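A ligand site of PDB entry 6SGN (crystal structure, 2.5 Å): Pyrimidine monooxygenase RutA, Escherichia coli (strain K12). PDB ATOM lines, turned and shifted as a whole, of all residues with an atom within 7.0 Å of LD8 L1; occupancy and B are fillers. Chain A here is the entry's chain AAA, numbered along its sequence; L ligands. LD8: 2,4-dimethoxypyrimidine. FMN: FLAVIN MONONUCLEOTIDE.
N of Ile 49 sits at hydrogen-bond distance from O4 of FMN L2 (3.0 Å). A nitrogen (N3) of FMN L2 lies within hydrogen-bond range of the backbone carbonyl oxygen of Ile 49 (3.4 Å). The indole nitrogen of Trp 14 is in hydrogen-bond range of an oxygen (O01) of LD8 L1 (3.3 Å). O02 of LD8 L1 sits close to NZ of Lys 50, at 3.4 Å.
N of Met 301 is in hydrogen-bond range of OD1 of Asn 298, 3.5 Å away. OE1 of Gln 121 lies close to NE1 of Trp 120 (3.3 Å). The side-chain sulfur of Met 301 lies within hydrogen-bond range of the side-chain hydroxyl of Thr 330 (3.5 Å).
CE of Met 48 touches O02 of LD8 L1 (3.3 Å). NE1 of Trp 120 touches C10 of LD8 L1, at 2.8 Å. Phe 207 touches LD8 L1. CD2 of Leu 240 touches C09 of LD8 L1 (3.999 Å). Met 301 touches LD8 L1. Hydrophobic or aromatic side chains within 4 Å of LD8 L1: Trp 14, Met 48, Trp 120, Phe 207, Leu 240 and Met 301. Of the 19 residues printed, 7 come within 4 Å of LD8 L1. The nearest printed residue that does not touch LD8 L1 is Trp 61 (4.002 Å).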
ATOM      1  N   PHE A   6      21.166  36.602  -5.796  1.00  0.00           N
ATOM      2  CA  PHE A   6      19.853  36.070  -5.554  1.00  0.00           C
ATOM      3  C   PHE A   6      19.185  36.947  -4.500  1.00  0.00           C
ATOM      4  O   PHE A   6      19.371  36.724  -3.304  1.00  0.00           O
ATOM      5  CB  PHE A   6      20.025  34.612  -5.118  1.00  0.00           C
ATOM      6  CG  PHE A   6      18.881  33.685  -5.392  1.00  0.00           C
ATOM      7  CD1 PHE A   6      17.900  34.004  -6.311  1.00  0.00           C
ATOM      8  CD2 PHE A   6      18.801  32.461  -4.748  1.00  0.00           C
ATOM      9  CE1 PHE A   6      16.852  33.135  -6.553  1.00  0.00           C
ATOM     10  CE2 PHE A   6      17.776  31.580  -5.022  1.00  0.00           C
ATOM     11  CZ  PHE A   6      16.785  31.927  -5.906  1.00  0.00           C
ATOM     12  N   TRP A  14      18.208  33.543   3.029  1.00  0.00           N
ATOM     13  CA  TRP A  14      18.313  32.093   2.909  1.00  0.00           C
ATOM     14  C   TRP A  14      18.867  31.468   4.178  1.00  0.00           C
ATOM     15  O   TRP A  14      19.448  30.386   4.125  1.00  0.00           O
ATOM     16  CB  TRP A  14      19.074  31.671   1.639  1.00  0.00           C
ATOM     17  CG  TRP A  14      18.181  31.719   0.447  1.00  0.00           C
ATOM     18  CD1 TRP A  14      17.461  30.702  -0.095  1.00  0.00           C
ATOM     19  CD2 TRP A  14      17.872  32.887  -0.340  1.00  0.00           C
ATOM     20  NE1 TRP A  14      16.736  31.140  -1.165  1.00  0.00           N
ATOM     21  CE2 TRP A  14      16.956  32.481  -1.331  1.00  0.00           C
ATOM     22  CE3 TRP A  14      18.295  34.225  -0.289  1.00  0.00           C
ATOM     23  CZ2 TRP A  14      16.454  33.381  -2.280  1.00  0.00           C
ATOM     24  CZ3 TRP A  14      17.796  35.107  -1.223  1.00  0.00           C
ATOM     25  CH2 TRP A  14      16.887  34.680  -2.207  1.00  0.00           C
ATOM     26  N   MET A  48      13.578  34.789  -6.917  1.00  0.00           N
ATOM     27  CA  MET A  48      12.582  33.720  -6.899  1.00  0.00           C
ATOM     28  C   MET A  48      11.153  34.266  -6.748  1.00  0.00           C
ATOM     29  O   MET A  48      10.913  35.475  -6.769  1.00  0.00           O
ATOM     30  CB  MET A  48      12.846  32.753  -5.744  1.00  0.00           C
ATOM     31  CG  MET A  48      12.681  33.395  -4.367  1.00  0.00           C
ATOM     32  SD  MET A  48      12.986  32.193  -2.995  1.00  0.00           S
ATOM     33  CE  MET A  48      11.853  30.914  -3.539  1.00  0.00           C
ATOM     34  N   ILE A  49      10.209  33.320  -6.639  1.00  0.00           N
ATOM     35  CA  ILE A  49       8.856  33.555  -6.169  1.00  0.00           C
ATOM     36  C   ILE A  49       8.554  32.491  -5.127  1.00  0.00           C
ATOM     37  O   ILE A  49       8.933  31.325  -5.306  1.00  0.00           O
ATOM     38  CB  ILE A  49       7.838  33.504  -7.332  1.00  0.00           C
ATOM     39  CG1 ILE A  49       6.487  34.143  -6.977  1.00  0.00           C
ATOM     40  CG2 ILE A  49       7.666  32.082  -7.813  1.00  0.00           C
ATOM     41  CD1 ILE A  49       6.461  35.649  -7.008  1.00  0.00           C
ATOM     42  N   LYS A  50       7.887  32.886  -4.043  1.00  0.00           N
ATOM     43  CA  LYS A  50       7.497  31.958  -2.982  1.00  0.00           C
ATOM     44  C   LYS A  50       6.134  32.325  -2.405  1.00  0.00           C
ATOM     45  O   LYS A  50       5.979  33.330  -1.702  1.00  0.00           O
ATOM     46  CB  LYS A  50       8.613  31.833  -1.948  1.00  0.00           C
ATOM     47  CG  LYS A  50       8.410  30.727  -0.913  1.00  0.00           C
ATOM     48  CD  LYS A  50       8.070  29.389  -1.510  1.00  0.00           C
ATOM     49  CE  LYS A  50       9.223  28.773  -2.269  1.00  0.00           C
ATOM     50  NZ  LYS A  50      10.321  28.383  -1.356  1.00  0.00           N
ATOM     51  N   PHE A  54       7.209  28.824   5.790  1.00  0.00           N
ATOM     52  CA  PHE A  54       7.452  27.619   6.578  1.00  0.00           C
ATOM     53  C   PHE A  54       7.267  27.885   8.070  1.00  0.00           C
ATOM     54  O   PHE A  54       7.581  27.023   8.890  1.00  0.00           O
ATOM     55  CB  PHE A  54       8.852  27.077   6.327  1.00  0.00           C
ATOM     56  CG  PHE A  54       9.147  26.856   4.875  1.00  0.00           C
ATOM     57  CD1 PHE A  54       8.531  25.823   4.171  1.00  0.00           C
ATOM     58  CD2 PHE A  54      10.012  27.706   4.189  1.00  0.00           C
ATOM     59  CE1 PHE A  54       8.790  25.639   2.818  1.00  0.00           C
ATOM     60  CE2 PHE A  54      10.261  27.516   2.844  1.00  0.00           C
ATOM     61  CZ  PHE A  54       9.661  26.479   2.159  1.00  0.00           C
ATOM     62  N   TRP A  61      10.093  32.878   5.312  1.00  0.00           N
ATOM     63  CA  TRP A  61       9.466  33.030   4.009  1.00  0.00           C
ATOM     64  C   TRP A  61       7.949  33.103   4.128  1.00  0.00           C
ATOM     65  O   TRP A  61       7.233  32.671   3.215  1.00  0.00           O
ATOM     66  CB  TRP A  61       9.918  31.937   3.028  1.00  0.00           C
ATOM     67  CG  TRP A  61      11.303  32.123   2.496  1.00  0.00           C
ATOM     68  CD1 TRP A  61      12.137  33.182   2.751  1.00  0.00           C
ATOM     69  CD2 TRP A  61      12.001  31.257   1.595  1.00  0.00           C
ATOM     70  NE1 TRP A  61      13.323  33.006   2.092  1.00  0.00           N
ATOM     71  CE2 TRP A  61      13.270  31.848   1.370  1.00  0.00           C
ATOM     72  CE3 TRP A  61      11.705  30.031   0.978  1.00  0.00           C
ATOM     73  CZ2 TRP A  61      14.229  31.251   0.537  1.00  0.00           C
ATOM     74  CZ3 TRP A  61      12.656  29.450   0.161  1.00  0.00           C
ATOM     75  CH2 TRP A  61      13.902  30.048  -0.064  1.00  0.00           C
ATOM     76  N   VAL A 117       9.423  28.494 -14.131  1.00  0.00           N
ATOM     77  CA  VAL A 117       9.371  27.596 -12.988  1.00  0.00           C
ATOM     78  C   VAL A 117       8.058  26.807 -13.046  1.00  0.00           C
ATOM     79  O   VAL A 117       6.988  27.364 -13.328  1.00  0.00           O
ATOM     80  CB  VAL A 117       9.582  28.386 -11.684  1.00  0.00           C
ATOM     81  CG1 VAL A 117       8.600  28.062 -10.568  1.00  0.00           C
ATOM     82  CG2 VAL A 117      11.032  28.326 -11.187  1.00  0.00           C
ATOM     83  N   GLY A 119       6.828  25.113 -10.438  1.00  0.00           N
ATOM     84  CA  GLY A 119       6.231  24.967  -9.122  1.00  0.00           C
ATOM     85  C   GLY A 119       6.416  23.539  -8.631  1.00  0.00           C
ATOM     86  O   GLY A 119       6.164  22.608  -9.384  1.00  0.00           O
ATOM     87  N   TRP A 120       6.887  23.359  -7.389  1.00  0.00           N
ATOM     88  CA  TRP A 120       7.176  22.018  -6.911  1.00  0.00           C
ATOM     89  C   TRP A 120       6.285  21.620  -5.735  1.00  0.00           C
ATOM     90  O   TRP A 120       5.745  20.516  -5.740  1.00  0.00           O
ATOM     91  CB  TRP A 120       8.686  21.808  -6.640  1.00  0.00           C
ATOM     92  CG  TRP A 120       9.228  22.571  -5.467  1.00  0.00           C
ATOM     93  CD1 TRP A 120       9.132  23.915  -5.251  1.00  0.00           C
ATOM     94  CD2 TRP A 120       9.988  22.032  -4.366  1.00  0.00           C
ATOM     95  NE1 TRP A 120       9.752  24.244  -4.077  1.00  0.00           N
ATOM     96  CE2 TRP A 120      10.294  23.123  -3.517  1.00  0.00           C
ATOM     97  CE3 TRP A 120      10.434  20.754  -4.008  1.00  0.00           C
ATOM     98  CZ2 TRP A 120      11.023  22.962  -2.332  1.00  0.00           C
ATOM     99  CZ3 TRP A 120      11.155  20.590  -2.838  1.00  0.00           C
ATOM    100  CH2 TRP A 120      11.449  21.685  -2.016  1.00  0.00           C
ATOM    101  N   GLN A 121       6.133  22.527  -4.754  1.00  0.00           N
ATOM    102  CA  GLN A 121       5.333  22.275  -3.573  1.00  0.00           C
ATOM    103  C   GLN A 121       3.845  22.488  -3.879  1.00  0.00           C
ATOM    104  O   GLN A 121       3.450  23.541  -4.390  1.00  0.00           O
ATOM    105  CB  GLN A 121       5.669  23.230  -2.427  1.00  0.00           C
ATOM    106  CG  GLN A 121       7.108  23.158  -1.955  1.00  0.00           C
ATOM    107  CD  GLN A 121       7.471  24.424  -1.229  1.00  0.00           C
ATOM    108  OE1 GLN A 121       8.645  24.697  -0.975  1.00  0.00           O
ATOM    109  NE2 GLN A 121       6.471  25.216  -0.870  1.00  0.00           N
ATOM    110  N   GLU A 124       1.692  25.669  -2.121  1.00  0.00           N
ATOM    111  CA  GLU A 124       1.732  26.978  -2.762  1.00  0.00           C
ATOM    112  C   GLU A 124       0.481  27.198  -3.637  1.00  0.00           C
ATOM    113  O   GLU A 124      -0.049  28.309  -3.677  1.00  0.00           O
ATOM    114  CB  GLU A 124       3.033  27.169  -3.559  1.00  0.00           C
ATOM    115  CG  GLU A 124       4.260  27.462  -2.706  1.00  0.00           C
ATOM    116  CD  GLU A 124       5.551  27.783  -3.451  1.00  0.00           C
ATOM    117  OE1 GLU A 124       5.599  28.846  -4.150  1.00  0.00           O
ATOM    118  OE2 GLU A 124       6.505  26.978  -3.356  1.00  0.00           O
ATOM    119  N   PHE A 207      22.089  23.700  -8.174  1.00  0.00           N
ATOM    120  CA  PHE A 207      22.516  23.927  -6.803  1.00  0.00           C
ATOM    121  C   PHE A 207      23.997  23.581  -6.656  1.00  0.00           C
ATOM    122  O   PHE A 207      24.384  22.493  -7.063  1.00  0.00           O
ATOM    123  CB  PHE A 207      21.688  23.071  -5.850  1.00  0.00           C
ATOM    124  CG  PHE A 207      20.202  23.338  -5.910  1.00  0.00           C
ATOM    125  CD1 PHE A 207      19.663  24.500  -5.371  1.00  0.00           C
ATOM    126  CD2 PHE A 207      19.352  22.433  -6.535  1.00  0.00           C
ATOM    127  CE1 PHE A 207      18.299  24.733  -5.441  1.00  0.00           C
ATOM    128  CE2 PHE A 207      17.981  22.686  -6.611  1.00  0.00           C
ATOM    129  CZ  PHE A 207      17.462  23.829  -6.060  1.00  0.00           C
ATOM    130  N   LEU A 240      24.215  27.896  -7.700  1.00  0.00           N
ATOM    131  CA  LEU A 240      23.854  28.628  -6.484  1.00  0.00           C
ATOM    132  C   LEU A 240      24.731  28.222  -5.288  1.00  0.00           C
ATOM    133  O   LEU A 240      24.810  27.038  -4.912  1.00  0.00           O
ATOM    134  CB  LEU A 240      22.389  28.372  -6.194  1.00  0.00           C
ATOM    135  CG  LEU A 240      21.893  28.814  -4.805  1.00  0.00           C
ATOM    136  CD1 LEU A 240      21.695  30.325  -4.733  1.00  0.00           C
ATOM    137  CD2 LEU A 240      20.595  28.118  -4.466  1.00  0.00           C
ATOM    138  N   LEU A 271       9.514  22.146   6.037  1.00  0.00           N
ATOM    139  CA  LEU A 271      10.222  21.854   4.791  1.00  0.00           C
ATOM    140  C   LEU A 271      10.174  20.357   4.493  1.00  0.00           C
ATOM    141  O   LEU A 271       9.938  19.965   3.349  1.00  0.00           O
ATOM    142  CB  LEU A 271      11.661  22.396   4.896  1.00  0.00           C
ATOM    143  CG  LEU A 271      11.947  23.722   4.191  1.00  0.00           C
ATOM    144  CD1 LEU A 271      12.866  24.610   5.011  1.00  0.00           C
ATOM    145  CD2 LEU A 271      12.523  23.491   2.803  1.00  0.00           C
ATOM    146  N   ASN A 298      20.302  26.554   5.720  1.00  0.00           N
ATOM    147  CA  ASN A 298      20.225  27.265   4.463  1.00  0.00           C
ATOM    148  C   ASN A 298      19.705  26.304   3.395  1.00  0.00           C
ATOM    149  O   ASN A 298      20.071  26.427   2.238  1.00  0.00           O
ATOM    150  CB  ASN A 298      21.531  28.001   4.155  1.00  0.00           C
ATOM    151  CG  ASN A 298      22.722  27.092   3.971  1.00  0.00           C
ATOM    152  OD1 ASN A 298      22.674  25.881   4.156  1.00  0.00           O
ATOM    153  ND2 ASN A 298      23.825  27.710   3.584  1.00  0.00           N
ATOM    154  N   ILE A 299      18.827  25.383   3.823  1.00  0.00           N
ATOM    155  CA  ILE A 299      18.140  24.412   2.981  1.00  0.00           C
ATOM    156  C   ILE A 299      19.174  23.506   2.315  1.00  0.00           C
ATOM    157  O   ILE A 299      19.006  23.127   1.152  1.00  0.00           O
ATOM    158  CB  ILE A 299      17.179  25.065   1.954  1.00  0.00           C
ATOM    159  CG1 ILE A 299      16.489  26.330   2.481  1.00  0.00           C
ATOM    160  CG2 ILE A 299      16.173  24.045   1.436  1.00  0.00           C
ATOM    161  CD1 ILE A 299      15.854  27.194   1.416  1.00  0.00           C
ATOM    162  N   MET A 301      22.026  24.217   1.202  1.00  0.00           N
ATOM    163  CA  MET A 301      22.666  24.916   0.105  1.00  0.00           C
ATOM    164  C   MET A 301      24.163  24.615   0.088  1.00  0.00           C
ATOM    165  O   MET A 301      24.751  24.264   1.099  1.00  0.00           O
ATOM    166  CB  MET A 301      22.487  26.434   0.260  1.00  0.00           C
ATOM    167  CG  MET A 301      22.693  27.205  -1.029  1.00  0.00           C
ATOM    168  SD  MET A 301      22.221  28.949  -0.845  1.00  0.00           S
ATOM    169  CE  MET A 301      20.468  28.813  -0.475  1.00  0.00           C
ATOM    170  N   THR A 330      24.039  33.951  -2.723  1.00  0.00           N
ATOM    171  CA  THR A 330      23.402  34.485  -1.538  1.00  0.00           C
ATOM    172  C   THR A 330      24.464  34.757  -0.478  1.00  0.00           C
ATOM    173  O   THR A 330      25.576  34.232  -0.534  1.00  0.00           O
ATOM    174  CB  THR A 330      22.335  33.537  -1.032  1.00  0.00           C
ATOM    175  OG1 THR A 330      23.014  32.333  -0.696  1.00  0.00           O
ATOM    176  CG2 THR A 330      21.298  33.231  -2.088  1.00  0.00           C
HETATM  177  O01 LD8 L   1      16.117  28.475  -3.003  1.00  0.00           O
HETATM  178  O02 LD8 L   1      11.723  27.757  -4.429  1.00  0.00           O
HETATM  179  N03 LD8 L   1      13.912  28.199  -3.732  1.00  0.00           N
HETATM  180  N04 LD8 L   1      13.128  25.793  -3.992  1.00  0.00           N
HETATM  181  C05 LD8 L   1      15.113  27.656  -3.343  1.00  0.00           C
HETATM  182  C06 LD8 L   1      15.391  26.216  -3.250  1.00  0.00           C
HETATM  183  C07 LD8 L   1      12.937  27.228  -4.037  1.00  0.00           C
HETATM  184  C08 LD8 L   1      14.359  25.340  -3.583  1.00  0.00           C
HETATM  185  C09 LD8 L   1      17.220  27.816  -2.342  1.00  0.00           C
HETATM  186  C10 LD8 L   1      10.562  26.932  -4.287  1.00  0.00           C
HETATM  187  N1  FMN L   2      11.195  26.878  -7.594  1.00  0.00           N
HETATM  188  C2  FMN L   2      10.108  27.723  -7.465  1.00  0.00           C
HETATM  189  O2  FMN L   2       8.957  27.269  -7.299  1.00  0.00           O
HETATM  190  N3  FMN L   2      10.231  29.067  -7.508  1.00  0.00           N
HETATM  191  C4  FMN L   2      11.435  29.650  -7.683  1.00  0.00           C
HETATM  192  O4  FMN L   2      11.567  30.884  -7.738  1.00  0.00           O
HETATM  193  C4A FMN L   2      12.649  28.834  -7.828  1.00  0.00           C
HETATM  194  N5  FMN L   2      13.833  29.423  -8.012  1.00  0.00           N
HETATM  195  C5A FMN L   2      14.944  28.664  -8.143  1.00  0.00           C
HETATM  196  C6  FMN L   2      16.181  29.289  -8.332  1.00  0.00           C
HETATM  197  C7  FMN L   2      17.343  28.562  -8.447  1.00  0.00           C
HETATM  198  C7M FMN L   2      18.637  29.287  -8.649  1.00  0.00           C
HETATM  199  C8  FMN L   2      17.351  27.081  -8.395  1.00  0.00           C
HETATM  200  C8M FMN L   2      18.675  26.345  -8.549  1.00  0.00           C
HETATM  201  C9  FMN L   2      16.112  26.433  -8.214  1.00  0.00           C
HETATM  202  C9A FMN L   2      14.889  27.153  -8.080  1.00  0.00           C
HETATM  203  N10 FMN L   2      13.609  26.512  -7.895  1.00  0.00           N
HETATM  204  C10 FMN L   2      12.464  27.345  -7.789  1.00  0.00           C
HETATM  205  C1' FMN L   2      13.460  25.046  -7.856  1.00  0.00           C
HETATM  206  C2' FMN L   2      13.492  24.503  -9.304  1.00  0.00           C
HETATM  207  O2' FMN L   2      12.623  25.305 -10.140  1.00  0.00           O
HETATM  208  C3' FMN L   2      13.208  22.983  -9.488  1.00  0.00           C
HETATM  209  O3' FMN L   2      11.896  22.691  -8.998  1.00  0.00           O
HETATM  210  C4' FMN L   2      14.201  21.958  -8.852  1.00  0.00           C
HETATM  211  O4' FMN L   2      15.576  22.411  -8.891  1.00  0.00           O
HETATM  212  C5' FMN L   2      14.009  20.481  -9.310  1.00  0.00           C
HETATM  213  O5' FMN L   2      14.131  20.230 -10.743  1.00  0.00           O
HETATM  214  P   FMN L   2      12.920  19.651 -11.688  1.00  0.00           P
HETATM  215  O1P FMN L   2      12.479  18.391 -10.993  1.00  0.00           O
HETATM  216  O2P FMN L   2      11.881  20.744 -11.676  1.00  0.00           O
HETATM  217  O3P FMN L   2      13.513  19.374 -13.051  1.00  0.00           O
